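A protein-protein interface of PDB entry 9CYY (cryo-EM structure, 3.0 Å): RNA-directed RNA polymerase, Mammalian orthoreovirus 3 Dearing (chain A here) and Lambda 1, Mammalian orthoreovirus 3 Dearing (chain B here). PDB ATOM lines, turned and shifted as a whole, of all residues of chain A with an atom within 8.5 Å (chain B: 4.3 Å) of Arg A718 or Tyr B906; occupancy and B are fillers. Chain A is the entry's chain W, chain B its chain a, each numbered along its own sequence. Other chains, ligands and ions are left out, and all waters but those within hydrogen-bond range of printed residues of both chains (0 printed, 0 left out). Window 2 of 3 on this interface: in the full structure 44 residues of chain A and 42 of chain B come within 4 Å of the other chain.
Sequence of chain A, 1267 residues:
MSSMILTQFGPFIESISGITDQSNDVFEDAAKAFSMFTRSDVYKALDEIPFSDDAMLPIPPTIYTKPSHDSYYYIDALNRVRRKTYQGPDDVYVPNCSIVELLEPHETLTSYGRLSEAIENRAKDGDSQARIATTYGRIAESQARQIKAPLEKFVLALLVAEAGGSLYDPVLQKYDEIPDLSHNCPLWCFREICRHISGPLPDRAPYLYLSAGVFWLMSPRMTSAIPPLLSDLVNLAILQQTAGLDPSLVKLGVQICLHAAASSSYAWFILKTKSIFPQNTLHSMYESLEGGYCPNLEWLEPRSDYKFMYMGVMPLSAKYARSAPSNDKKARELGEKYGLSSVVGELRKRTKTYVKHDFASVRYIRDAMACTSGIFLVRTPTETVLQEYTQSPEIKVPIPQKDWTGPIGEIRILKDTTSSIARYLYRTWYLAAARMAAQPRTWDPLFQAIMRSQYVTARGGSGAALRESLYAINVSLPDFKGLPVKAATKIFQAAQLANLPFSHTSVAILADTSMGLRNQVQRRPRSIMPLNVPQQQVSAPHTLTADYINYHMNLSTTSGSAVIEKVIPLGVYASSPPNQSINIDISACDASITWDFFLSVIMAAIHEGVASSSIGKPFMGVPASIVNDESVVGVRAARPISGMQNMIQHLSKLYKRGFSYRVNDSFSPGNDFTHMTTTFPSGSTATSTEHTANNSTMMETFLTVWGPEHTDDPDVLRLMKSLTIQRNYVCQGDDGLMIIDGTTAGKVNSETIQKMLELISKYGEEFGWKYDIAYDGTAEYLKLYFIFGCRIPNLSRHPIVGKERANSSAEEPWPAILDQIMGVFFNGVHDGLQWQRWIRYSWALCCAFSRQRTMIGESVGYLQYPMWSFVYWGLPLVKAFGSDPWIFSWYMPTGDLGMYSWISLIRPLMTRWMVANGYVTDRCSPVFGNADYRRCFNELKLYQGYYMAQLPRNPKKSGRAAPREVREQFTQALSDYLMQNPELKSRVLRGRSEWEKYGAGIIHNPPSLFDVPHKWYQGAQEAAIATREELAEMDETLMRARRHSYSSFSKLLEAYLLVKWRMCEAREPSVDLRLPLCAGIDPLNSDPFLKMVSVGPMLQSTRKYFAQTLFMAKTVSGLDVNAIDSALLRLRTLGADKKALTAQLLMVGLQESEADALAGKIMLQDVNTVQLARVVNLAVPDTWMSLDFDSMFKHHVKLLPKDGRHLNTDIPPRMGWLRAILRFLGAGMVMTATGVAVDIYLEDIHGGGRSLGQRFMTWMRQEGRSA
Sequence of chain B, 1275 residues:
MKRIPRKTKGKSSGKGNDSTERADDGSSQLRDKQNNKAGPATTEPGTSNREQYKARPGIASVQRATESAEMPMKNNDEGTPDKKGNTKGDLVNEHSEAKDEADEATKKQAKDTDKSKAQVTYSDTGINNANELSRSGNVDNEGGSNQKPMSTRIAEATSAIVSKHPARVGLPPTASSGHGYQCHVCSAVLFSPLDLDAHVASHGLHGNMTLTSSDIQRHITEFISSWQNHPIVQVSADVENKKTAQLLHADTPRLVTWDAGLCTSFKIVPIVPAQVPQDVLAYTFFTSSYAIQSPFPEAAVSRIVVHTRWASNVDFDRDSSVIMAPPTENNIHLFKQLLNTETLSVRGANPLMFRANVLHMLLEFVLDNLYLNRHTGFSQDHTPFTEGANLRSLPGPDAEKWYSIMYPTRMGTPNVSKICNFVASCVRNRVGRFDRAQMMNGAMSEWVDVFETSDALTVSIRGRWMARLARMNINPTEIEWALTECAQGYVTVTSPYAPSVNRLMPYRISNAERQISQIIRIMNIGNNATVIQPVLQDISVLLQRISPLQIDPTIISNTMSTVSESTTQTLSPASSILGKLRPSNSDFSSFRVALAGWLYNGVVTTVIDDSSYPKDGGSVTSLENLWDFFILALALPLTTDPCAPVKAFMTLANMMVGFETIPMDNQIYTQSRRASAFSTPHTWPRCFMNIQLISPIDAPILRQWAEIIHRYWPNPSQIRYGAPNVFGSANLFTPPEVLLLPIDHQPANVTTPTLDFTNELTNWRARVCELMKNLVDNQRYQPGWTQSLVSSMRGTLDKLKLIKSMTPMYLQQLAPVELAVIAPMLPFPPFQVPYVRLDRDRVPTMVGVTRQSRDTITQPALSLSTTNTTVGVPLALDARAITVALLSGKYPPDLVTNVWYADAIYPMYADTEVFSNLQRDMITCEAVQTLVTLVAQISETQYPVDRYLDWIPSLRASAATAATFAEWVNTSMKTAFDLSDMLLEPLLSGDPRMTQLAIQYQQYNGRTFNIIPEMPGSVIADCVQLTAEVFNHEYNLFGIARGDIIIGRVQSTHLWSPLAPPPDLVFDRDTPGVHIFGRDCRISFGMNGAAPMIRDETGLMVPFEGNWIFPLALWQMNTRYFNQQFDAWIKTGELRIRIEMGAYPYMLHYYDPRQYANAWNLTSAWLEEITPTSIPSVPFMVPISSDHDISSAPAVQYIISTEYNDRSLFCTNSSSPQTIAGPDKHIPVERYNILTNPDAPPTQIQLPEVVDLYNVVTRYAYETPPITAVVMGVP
The backbone carbonyl oxygen (O) of Asp B903 is in hydrogen-bond range of the guanidinium group (NH2) of Arg A718 (3.2 Å). OG1 of Thr A744 sits at hydrogen-bond distance from O of Ala B904 (3.2 Å).
Arg A718 touches three residues of chain B. Printed residues of chain A within 4 Å of Asp B903: Arg A718 (3.2 Å). Of the printed residues of chain B, Thr A743 touches Pro B907 (3.97 Å). Of the printed residues of chain A, Ala B904 touches Thr A744. Of the printed residues of chain B, Ala A745 touches Pro B907. Of the printed residues of chain A, Met B908 touches Thr A744. Val A748 touches none of the printed residues of chain B. The nearest residue of chain A that does not touch Tyr B906 is Asp A715 (6.0 Å). The nearest printed residue of chain B that does not touch Thr A743 is Ala B904 (6.1 Å).
Of the 12 printed residues of chain B, 5 touch a printed residue of chain A. Hydrophobic or aromatic side chains of chain B within 4 Å of the printed part of chain A: Tyr B906, Pro B907 and Met B908.
Arg A718 touches Tyr B906 (NE to CD2, 3.9 Å). Arg A718 touches Pro B907. CB of Pro B907 touches CB of Thr A743, 3.97 Å away. Pro B907 touches Thr A744. CG2 of Thr A744 touches CE of Met B908, 3.6 Å away. Ala A745 touches Pro B907 (CB to O, 3.8 Å).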
ATOM      1  N   PRO A 708     -10.769   8.773   9.785  1.00  0.00           N
ATOM      2  CA  PRO A 708      -9.355   9.114   9.561  1.00  0.00           C
ATOM      3  C   PRO A 708      -8.821   8.683   8.207  1.00  0.00           C
ATOM      4  O   PRO A 708      -7.866   9.303   7.722  1.00  0.00           O
ATOM      5  CB  PRO A 708      -8.631   8.394  10.706  1.00  0.00           C
ATOM      6  CG  PRO A 708      -9.669   8.222  11.755  1.00  0.00           C
ATOM      7  CD  PRO A 708     -10.946   7.991  11.021  1.00  0.00           C
ATOM      8  N   THR A 711     -10.807  11.441   5.577  1.00  0.00           N
ATOM      9  CA  THR A 711     -10.615  12.887   5.647  1.00  0.00           C
ATOM     10  C   THR A 711      -9.159  13.230   5.918  1.00  0.00           C
ATOM     11  O   THR A 711      -8.407  12.418   6.467  1.00  0.00           O
ATOM     12  CB  THR A 711     -11.484  13.543   6.723  1.00  0.00           C
ATOM     13  OG1 THR A 711     -11.374  14.966   6.614  1.00  0.00           O
ATOM     14  CG2 THR A 711     -11.022  13.137   8.105  1.00  0.00           C
ATOM     15  N   ASP A 712      -8.771  14.448   5.532  1.00  0.00           N
ATOM     16  CA  ASP A 712      -7.397  14.911   5.654  1.00  0.00           C
ATOM     17  C   ASP A 712      -7.245  16.249   6.365  1.00  0.00           C
ATOM     18  O   ASP A 712      -6.111  16.679   6.591  1.00  0.00           O
ATOM     19  CB  ASP A 712      -6.746  15.006   4.266  1.00  0.00           C
ATOM     20  CG  ASP A 712      -7.454  15.991   3.351  1.00  0.00           C
ATOM     21  OD1 ASP A 712      -8.482  16.570   3.763  1.00  0.00           O
ATOM     22  OD2 ASP A 712      -6.980  16.187   2.213  1.00  0.00           O
ATOM     23  N   ASP A 713      -8.341  16.914   6.712  1.00  0.00           N
ATOM     24  CA  ASP A 713      -8.252  18.199   7.386  1.00  0.00           C
ATOM     25  C   ASP A 713      -7.672  18.010   8.788  1.00  0.00           C
ATOM     26  O   ASP A 713      -8.218  17.226   9.576  1.00  0.00           O
ATOM     27  CB  ASP A 713      -9.632  18.852   7.468  1.00  0.00           C
ATOM     28  CG  ASP A 713      -9.581  20.253   8.039  1.00  0.00           C
ATOM     29  OD1 ASP A 713      -9.164  21.179   7.310  1.00  0.00           O
ATOM     30  OD2 ASP A 713      -9.961  20.432   9.215  1.00  0.00           O
ATOM     31  N   PRO A 714      -6.578  18.699   9.130  1.00  0.00           N
ATOM     32  CA  PRO A 714      -5.935  18.447  10.435  1.00  0.00           C
ATOM     33  C   PRO A 714      -6.844  18.695  11.627  1.00  0.00           C
ATOM     34  O   PRO A 714      -6.796  17.941  12.608  1.00  0.00           O
ATOM     35  CB  PRO A 714      -4.737  19.409  10.420  1.00  0.00           C
ATOM     36  CG  PRO A 714      -4.526  19.749   8.984  1.00  0.00           C
ATOM     37  CD  PRO A 714      -5.876  19.732   8.354  1.00  0.00           C
ATOM     38  N   ASP A 715      -7.675  19.737  11.568  1.00  0.00           N
ATOM     39  CA  ASP A 715      -8.591  20.007  12.670  1.00  0.00           C
ATOM     40  C   ASP A 715      -9.592  18.874  12.834  1.00  0.00           C
ATOM     41  O   ASP A 715      -9.882  18.445  13.958  1.00  0.00           O
ATOM     42  CB  ASP A 715      -9.312  21.332  12.437  1.00  0.00           C
ATOM     43  CG  ASP A 715      -8.388  22.524  12.546  1.00  0.00           C
ATOM     44  OD1 ASP A 715      -7.396  22.439  13.301  1.00  0.00           O
ATOM     45  OD2 ASP A 715      -8.648  23.543  11.876  1.00  0.00           O
ATOM     46  N   VAL A 716     -10.116  18.364  11.718  1.00  0.00           N
ATOM     47  CA  VAL A 716     -11.054  17.250  11.776  1.00  0.00           C
ATOM     48  C   VAL A 716     -10.370  16.013  12.344  1.00  0.00           C
ATOM     49  O   VAL A 716     -10.928  15.306  13.190  1.00  0.00           O
ATOM     50  CB  VAL A 716     -11.650  16.979  10.384  1.00  0.00           C
ATOM     51  CG1 VAL A 716     -12.401  15.660  10.372  1.00  0.00           C
ATOM     52  CG2 VAL A 716     -12.562  18.121   9.969  1.00  0.00           C
ATOM     53  N   LEU A 717      -9.144  15.735  11.889  1.00  0.00           N
ATOM     54  CA  LEU A 717      -8.408  14.584  12.404  1.00  0.00           C
ATOM     55  C   LEU A 717      -8.215  14.688  13.910  1.00  0.00           C
ATOM     56  O   LEU A 717      -8.436  13.718  14.644  1.00  0.00           O
ATOM     57  CB  LEU A 717      -7.053  14.455  11.703  1.00  0.00           C
ATOM     58  CG  LEU A 717      -6.942  13.630  10.419  1.00  0.00           C
ATOM     59  CD1 LEU A 717      -7.251  12.171  10.712  1.00  0.00           C
ATOM     60  CD2 LEU A 717      -7.840  14.152   9.319  1.00  0.00           C
ATOM     61  N   ARG A 718      -7.805  15.864  14.388  1.00  0.00           N
ATOM     62  CA  ARG A 718      -7.587  16.043  15.817  1.00  0.00           C
ATOM     63  C   ARG A 718      -8.887  15.876  16.593  1.00  0.00           C
ATOM     64  O   ARG A 718      -8.913  15.257  17.665  1.00  0.00           O
ATOM     65  CB  ARG A 718      -6.962  17.412  16.084  1.00  0.00           C
ATOM     66  CG  ARG A 718      -6.622  17.659  17.540  1.00  0.00           C
ATOM     67  CD  ARG A 718      -5.955  19.009  17.729  1.00  0.00           C
ATOM     68  NE  ARG A 718      -5.585  19.241  19.119  1.00  0.00           N
ATOM     69  CZ  ARG A 718      -6.371  19.811  20.022  1.00  0.00           C
ATOM     70  NH1 ARG A 718      -7.583  20.240  19.710  1.00  0.00           N
ATOM     71  NH2 ARG A 718      -5.931  19.954  21.268  1.00  0.00           N
ATOM     72  N   LEU A 719      -9.986  16.410  16.056  1.00  0.00           N
ATOM     73  CA  LEU A 719     -11.274  16.289  16.730  1.00  0.00           C
ATOM     74  C   LEU A 719     -11.694  14.827  16.853  1.00  0.00           C
ATOM     75  O   LEU A 719     -12.095  14.370  17.930  1.00  0.00           O
ATOM     76  CB  LEU A 719     -12.328  17.096  15.974  1.00  0.00           C
ATOM     77  CG  LEU A 719     -13.728  17.160  16.580  1.00  0.00           C
ATOM     78  CD1 LEU A 719     -13.653  17.697  17.997  1.00  0.00           C
ATOM     79  CD2 LEU A 719     -14.646  18.018  15.726  1.00  0.00           C
ATOM     80  N   MET A 720     -11.600  14.073  15.756  1.00  0.00           N
ATOM     81  CA  MET A 720     -11.999  12.667  15.793  1.00  0.00           C
ATOM     82  C   MET A 720     -11.079  11.842  16.685  1.00  0.00           C
ATOM     83  O   MET A 720     -11.534  10.902  17.349  1.00  0.00           O
ATOM     84  CB  MET A 720     -12.055  12.096  14.379  1.00  0.00           C
ATOM     85  CG  MET A 720     -12.756  13.002  13.385  1.00  0.00           C
ATOM     86  SD  MET A 720     -13.210  12.142  11.880  1.00  0.00           S
ATOM     87  CE  MET A 720     -11.599  11.520  11.437  1.00  0.00           C
ATOM     88  N   LYS A 721      -9.784  12.163  16.713  1.00  0.00           N
ATOM     89  CA  LYS A 721      -8.894  11.483  17.649  1.00  0.00           C
ATOM     90  C   LYS A 721      -9.284  11.783  19.090  1.00  0.00           C
ATOM     91  O   LYS A 721      -9.202  10.907  19.959  1.00  0.00           O
ATOM     92  CB  LYS A 721      -7.442  11.876  17.385  1.00  0.00           C
ATOM     93  CG  LYS A 721      -6.892  11.364  16.063  1.00  0.00           C
ATOM     94  CD  LYS A 721      -5.436  11.760  15.872  1.00  0.00           C
ATOM     95  CE  LYS A 721      -4.897  11.264  14.538  1.00  0.00           C
ATOM     96  NZ  LYS A 721      -3.476  11.656  14.329  1.00  0.00           N
ATOM     97  N   SER A 722      -9.709  13.019  19.367  1.00  0.00           N
ATOM     98  CA  SER A 722     -10.155  13.356  20.715  1.00  0.00           C
ATOM     99  C   SER A 722     -11.419  12.591  21.093  1.00  0.00           C
ATOM    100  O   SER A 722     -11.542  12.106  22.224  1.00  0.00           O
ATOM    101  CB  SER A 722     -10.383  14.862  20.830  1.00  0.00           C
ATOM    102  OG  SER A 722     -11.660  15.223  20.335  1.00  0.00           O
ATOM    103  N   LEU A 723     -12.367  12.474  20.167  1.00  0.00           N
ATOM    104  CA  LEU A 723     -13.631  11.804  20.455  1.00  0.00           C
ATOM    105  C   LEU A 723     -13.451  10.304  20.677  1.00  0.00           C
ATOM    106  O   LEU A 723     -12.560   9.668  20.108  1.00  0.00           O
ATOM    107  CB  LEU A 723     -14.645  12.036  19.332  1.00  0.00           C
ATOM    108  CG  LEU A 723     -15.521  13.292  19.360  1.00  0.00           C
ATOM    109  CD1 LEU A 723     -16.433  13.239  20.566  1.00  0.00           C
ATOM    110  CD2 LEU A 723     -14.727  14.572  19.391  1.00  0.00           C
ATOM    111  N   GLY A 742     -15.140  21.507  25.596  1.00  0.00           N
ATOM    112  CA  GLY A 742     -14.553  22.778  25.221  1.00  0.00           C
ATOM    113  C   GLY A 742     -13.041  22.781  25.345  1.00  0.00           C
ATOM    114  O   GLY A 742     -12.486  22.403  26.373  1.00  0.00           O
ATOM    115  N   THR A 743     -12.379  23.217  24.277  1.00  0.00           N
ATOM    116  CA  THR A 743     -10.935  23.367  24.279  1.00  0.00           C
ATOM    117  C   THR A 743     -10.562  24.619  25.065  1.00  0.00           C
ATOM    118  O   THR A 743     -11.411  25.451  25.390  1.00  0.00           O
ATOM    119  CB  THR A 743     -10.398  23.433  22.851  1.00  0.00           C
ATOM    120  OG1 THR A 743     -10.772  24.681  22.256  1.00  0.00           O
ATOM    121  CG2 THR A 743     -10.968  22.293  22.021  1.00  0.00           C
ATOM    122  N   THR A 744      -9.274  24.758  25.388  1.00  0.00           N
ATOM    123  CA  THR A 744      -8.833  25.846  26.255  1.00  0.00           C
ATOM    124  C   THR A 744      -9.135  27.220  25.669  1.00  0.00           C
ATOM    125  O   THR A 744      -9.280  28.185  26.429  1.00  0.00           O
ATOM    126  CB  THR A 744      -7.333  25.700  26.534  1.00  0.00           C
ATOM    127  OG1 THR A 744      -7.093  24.450  27.185  1.00  0.00           O
ATOM    128  CG2 THR A 744      -6.842  26.808  27.446  1.00  0.00           C
ATOM    129  N   ALA A 745      -9.294  27.323  24.352  1.00  0.00           N
ATOM    130  CA  ALA A 745      -9.604  28.586  23.695  1.00  0.00           C
ATOM    131  C   ALA A 745     -11.102  28.852  23.625  1.00  0.00           C
ATOM    132  O   ALA A 745     -11.525  29.779  22.927  1.00  0.00           O
ATOM    133  CB  ALA A 745      -8.999  28.612  22.291  1.00  0.00           C
ATOM    134  N   VAL A 748     -15.573  24.821  20.260  1.00  0.00           N
ATOM    135  CA  VAL A 748     -14.910  24.144  19.151  1.00  0.00           C
ATOM    136  C   VAL A 748     -15.358  24.771  17.835  1.00  0.00           C
ATOM    137  O   VAL A 748     -16.446  25.348  17.734  1.00  0.00           O
ATOM    138  CB  VAL A 748     -15.207  22.631  19.215  1.00  0.00           C
ATOM    139  CG1 VAL A 748     -14.608  21.884  18.033  1.00  0.00           C
ATOM    140  CG2 VAL A 748     -14.685  22.058  20.519  1.00  0.00           C
ATOM    141  N   THR A 752     -15.537  23.116  11.331  1.00  0.00           N
ATOM    142  CA  THR A 752     -14.887  21.825  11.539  1.00  0.00           C
ATOM    143  C   THR A 752     -15.899  20.778  11.986  1.00  0.00           C
ATOM    144  O   THR A 752     -15.952  19.663  11.442  1.00  0.00           O
ATOM    145  CB  THR A 752     -13.768  21.966  12.572  1.00  0.00           C
ATOM    146  OG1 THR A 752     -12.833  22.956  12.130  1.00  0.00           O
ATOM    147  CG2 THR A 752     -13.050  20.644  12.768  1.00  0.00           C
ATOM    148  N   MET A 756     -17.313  17.379   9.995  1.00  0.00           N
ATOM    149  CA  MET A 756     -17.495  16.071  10.608  1.00  0.00           C
ATOM    150  C   MET A 756     -18.920  15.558  10.396  1.00  0.00           C
ATOM    151  O   MET A 756     -19.133  14.352  10.229  1.00  0.00           O
ATOM    152  CB  MET A 756     -17.159  16.142  12.100  1.00  0.00           C
ATOM    153  CG  MET A 756     -17.064  14.781  12.765  1.00  0.00           C
ATOM    154  SD  MET A 756     -16.836  14.865  14.552  1.00  0.00           S
ATOM    155  CE  MET A 756     -18.334  14.064  15.123  1.00  0.00           C
ATOM    156  N   VAL B 491       4.562  22.481  24.038  1.00  0.00           N
ATOM    157  CA  VAL B 491       4.062  22.791  22.705  1.00  0.00           C
ATOM    158  C   VAL B 491       5.250  23.152  21.827  1.00  0.00           C
ATOM    159  O   VAL B 491       6.121  23.927  22.232  1.00  0.00           O
ATOM    160  CB  VAL B 491       3.032  23.939  22.735  1.00  0.00           C
ATOM    161  CG1 VAL B 491       2.692  24.388  21.326  1.00  0.00           C
ATOM    162  CG2 VAL B 491       1.777  23.508  23.472  1.00  0.00           C
ATOM    163  N   ALA B 902       0.405  18.117  26.648  1.00  0.00           N
ATOM    164  CA  ALA B 902       0.564  18.377  25.223  1.00  0.00           C
ATOM    165  C   ALA B 902      -0.789  18.464  24.534  1.00  0.00           C
ATOM    166  O   ALA B 902      -0.963  19.234  23.583  1.00  0.00           O
ATOM    167  CB  ALA B 902       1.426  17.292  24.583  1.00  0.00           C
ATOM    168  N   ASP B 903      -1.761  17.681  25.003  1.00  0.00           N
ATOM    169  CA  ASP B 903      -3.107  17.787  24.451  1.00  0.00           C
ATOM    170  C   ASP B 903      -3.816  19.042  24.952  1.00  0.00           C
ATOM    171  O   ASP B 903      -4.535  19.699  24.190  1.00  0.00           O
ATOM    172  CB  ASP B 903      -3.909  16.532  24.797  1.00  0.00           C
ATOM    173  CG  ASP B 903      -5.292  16.526  24.173  1.00  0.00           C
ATOM    174  OD1 ASP B 903      -6.143  17.347  24.574  1.00  0.00           O
ATOM    175  OD2 ASP B 903      -5.531  15.694  23.273  1.00  0.00           O
ATOM    176  N   ALA B 904      -3.624  19.395  26.226  1.00  0.00           N
ATOM    177  CA  ALA B 904      -4.436  20.448  26.831  1.00  0.00           C
ATOM    178  C   ALA B 904      -3.991  21.844  26.402  1.00  0.00           C
ATOM    179  O   ALA B 904      -4.815  22.647  25.957  1.00  0.00           O
ATOM    180  CB  ALA B 904      -4.399  20.325  28.353  1.00  0.00           C
ATOM    181  N   ILE B 905      -2.703  22.164  26.553  1.00  0.00           N
ATOM    182  CA  ILE B 905      -2.252  23.534  26.299  1.00  0.00           C
ATOM    183  C   ILE B 905      -2.304  23.930  24.825  1.00  0.00           C
ATOM    184  O   ILE B 905      -2.482  25.116  24.525  1.00  0.00           O
ATOM    185  CB  ILE B 905      -0.843  23.779  26.880  1.00  0.00           C
ATOM    186  CG1 ILE B 905      -0.838  23.647  28.407  1.00  0.00           C
ATOM    187  CG2 ILE B 905      -0.300  25.147  26.503  1.00  0.00           C
ATOM    188  CD1 ILE B 905      -0.586  22.285  28.944  1.00  0.00           C
ATOM    189  N   TYR B 906      -2.207  22.979  23.894  1.00  0.00           N
ATOM    190  CA  TYR B 906      -2.053  23.296  22.475  1.00  0.00           C
ATOM    191  C   TYR B 906      -3.065  24.316  21.948  1.00  0.00           C
ATOM    192  O   TYR B 906      -2.658  25.267  21.270  1.00  0.00           O
ATOM    193  CB  TYR B 906      -2.121  22.018  21.635  1.00  0.00           C
ATOM    194  CG  TYR B 906      -2.119  22.269  20.144  1.00  0.00           C
ATOM    195  CD1 TYR B 906      -0.928  22.439  19.452  1.00  0.00           C
ATOM    196  CD2 TYR B 906      -3.305  22.332  19.426  1.00  0.00           C
ATOM    197  CE1 TYR B 906      -0.921  22.670  18.093  1.00  0.00           C
ATOM    198  CE2 TYR B 906      -3.306  22.563  18.067  1.00  0.00           C
ATOM    199  CZ  TYR B 906      -2.112  22.730  17.405  1.00  0.00           C
ATOM    200  OH  TYR B 906      -2.108  22.959  16.050  1.00  0.00           O
ATOM    201  N   PRO B 907      -4.372  24.173  22.210  1.00  0.00           N
ATOM    202  CA  PRO B 907      -5.311  25.195  21.708  1.00  0.00           C
ATOM    203  C   PRO B 907      -5.068  26.585  22.271  1.00  0.00           C
ATOM    204  O   PRO B 907      -5.415  27.578  21.620  1.00  0.00           O
ATOM    205  CB  PRO B 907      -6.684  24.650  22.126  1.00  0.00           C
ATOM    206  CG  PRO B 907      -6.408  23.674  23.198  1.00  0.00           C
ATOM    207  CD  PRO B 907      -5.091  23.068  22.868  1.00  0.00           C
ATOM    208  N   MET B 908      -4.493  26.687  23.471  1.00  0.00           N
ATOM    209  CA  MET B 908      -4.329  27.990  24.108  1.00  0.00           C
ATOM    210  C   MET B 908      -3.367  28.887  23.340  1.00  0.00           C
ATOM    211  O   MET B 908      -3.594  30.097  23.243  1.00  0.00           O
ATOM    212  CB  MET B 908      -3.839  27.819  25.546  1.00  0.00           C
ATOM    213  CG  MET B 908      -3.693  29.127  26.307  1.00  0.00           C
ATOM    214  SD  MET B 908      -2.970  28.950  27.949  1.00  0.00           S
ATOM    215  CE  MET B 908      -3.415  27.266  28.355  1.00  0.00           C
ATOM    216  N   TYR B 909      -2.297  28.322  22.788  1.00  0.00           N
ATOM    217  CA  TYR B 909      -1.204  29.117  22.247  1.00  0.00           C
ATOM    218  C   TYR B 909      -1.368  29.457  20.772  1.00  0.00           C
ATOM    219  O   TYR B 909      -0.363  29.648  20.082  1.00  0.00           O
ATOM    220  CB  TYR B 909       0.128  28.397  22.472  1.00  0.00           C
ATOM    221  CG  TYR B 909       0.789  28.788  23.772  1.00  0.00           C
ATOM    222  CD1 TYR B 909       0.200  28.478  24.988  1.00  0.00           C
ATOM    223  CD2 TYR B 909       1.988  29.484  23.784  1.00  0.00           C
ATOM    224  CE1 TYR B 909       0.790  28.840  26.179  1.00  0.00           C
ATOM    225  CE2 TYR B 909       2.586  29.851  24.973  1.00  0.00           C
ATOM    226  CZ  TYR B 909       1.982  29.526  26.168  1.00  0.00           C
ATOM    227  OH  TYR B 909       2.571  29.887  27.356  1.00  0.00           O
ATOM    228  N   GLY B1273       2.217  25.494  14.532  1.00  0.00           N
ATOM    229  CA  GLY B1273       2.538  24.534  15.572  1.00  0.00           C
ATOM    230  C   GLY B1273       2.141  23.127  15.157  1.00  0.00           C
ATOM    231  O   GLY B1273       1.160  22.934  14.440  1.00  0.00           O
ATOM    232  N   VAL B1274       2.921  22.153  15.611  1.00  0.00           N
ATOM    233  CA  VAL B1274       2.629  20.748  15.343  1.00  0.00           C
ATOM    234  C   VAL B1274       1.448  20.334  16.211  1.00  0.00           C
ATOM    235  O   VAL B1274       1.518  20.447  17.443  1.00  0.00           O
ATOM    236  CB  VAL B1274       3.853  19.860  15.605  1.00  0.00           C
ATOM    237  CG1 VAL B1274       3.487  18.397  15.440  1.00  0.00           C
ATOM    238  CG2 VAL B1274       4.987  20.238  14.674  1.00  0.00           C
ATOM    239  N   PRO B1275       0.347  19.850  15.621  1.00  0.00           N
ATOM    240  CA  PRO B1275      -0.856  19.479  16.372  1.00  0.00           C
ATOM    241  C   PRO B1275      -0.619  18.303  17.311  1.00  0.00           C
ATOM    242  O   PRO B1275      -1.367  18.094  18.264  1.00  0.00           O
ATOM    243  CB  PRO B1275      -1.852  19.104  15.273  1.00  0.00           C
ATOM    244  CG  PRO B1275      -1.004  18.701  14.120  1.00  0.00           C
ATOM    245  CD  PRO B1275       0.200  19.585  14.180  1.00  0.00           C
ATOM    246  OXT PRO B1275       0.328  17.537  17.137  1.00  0.00           O
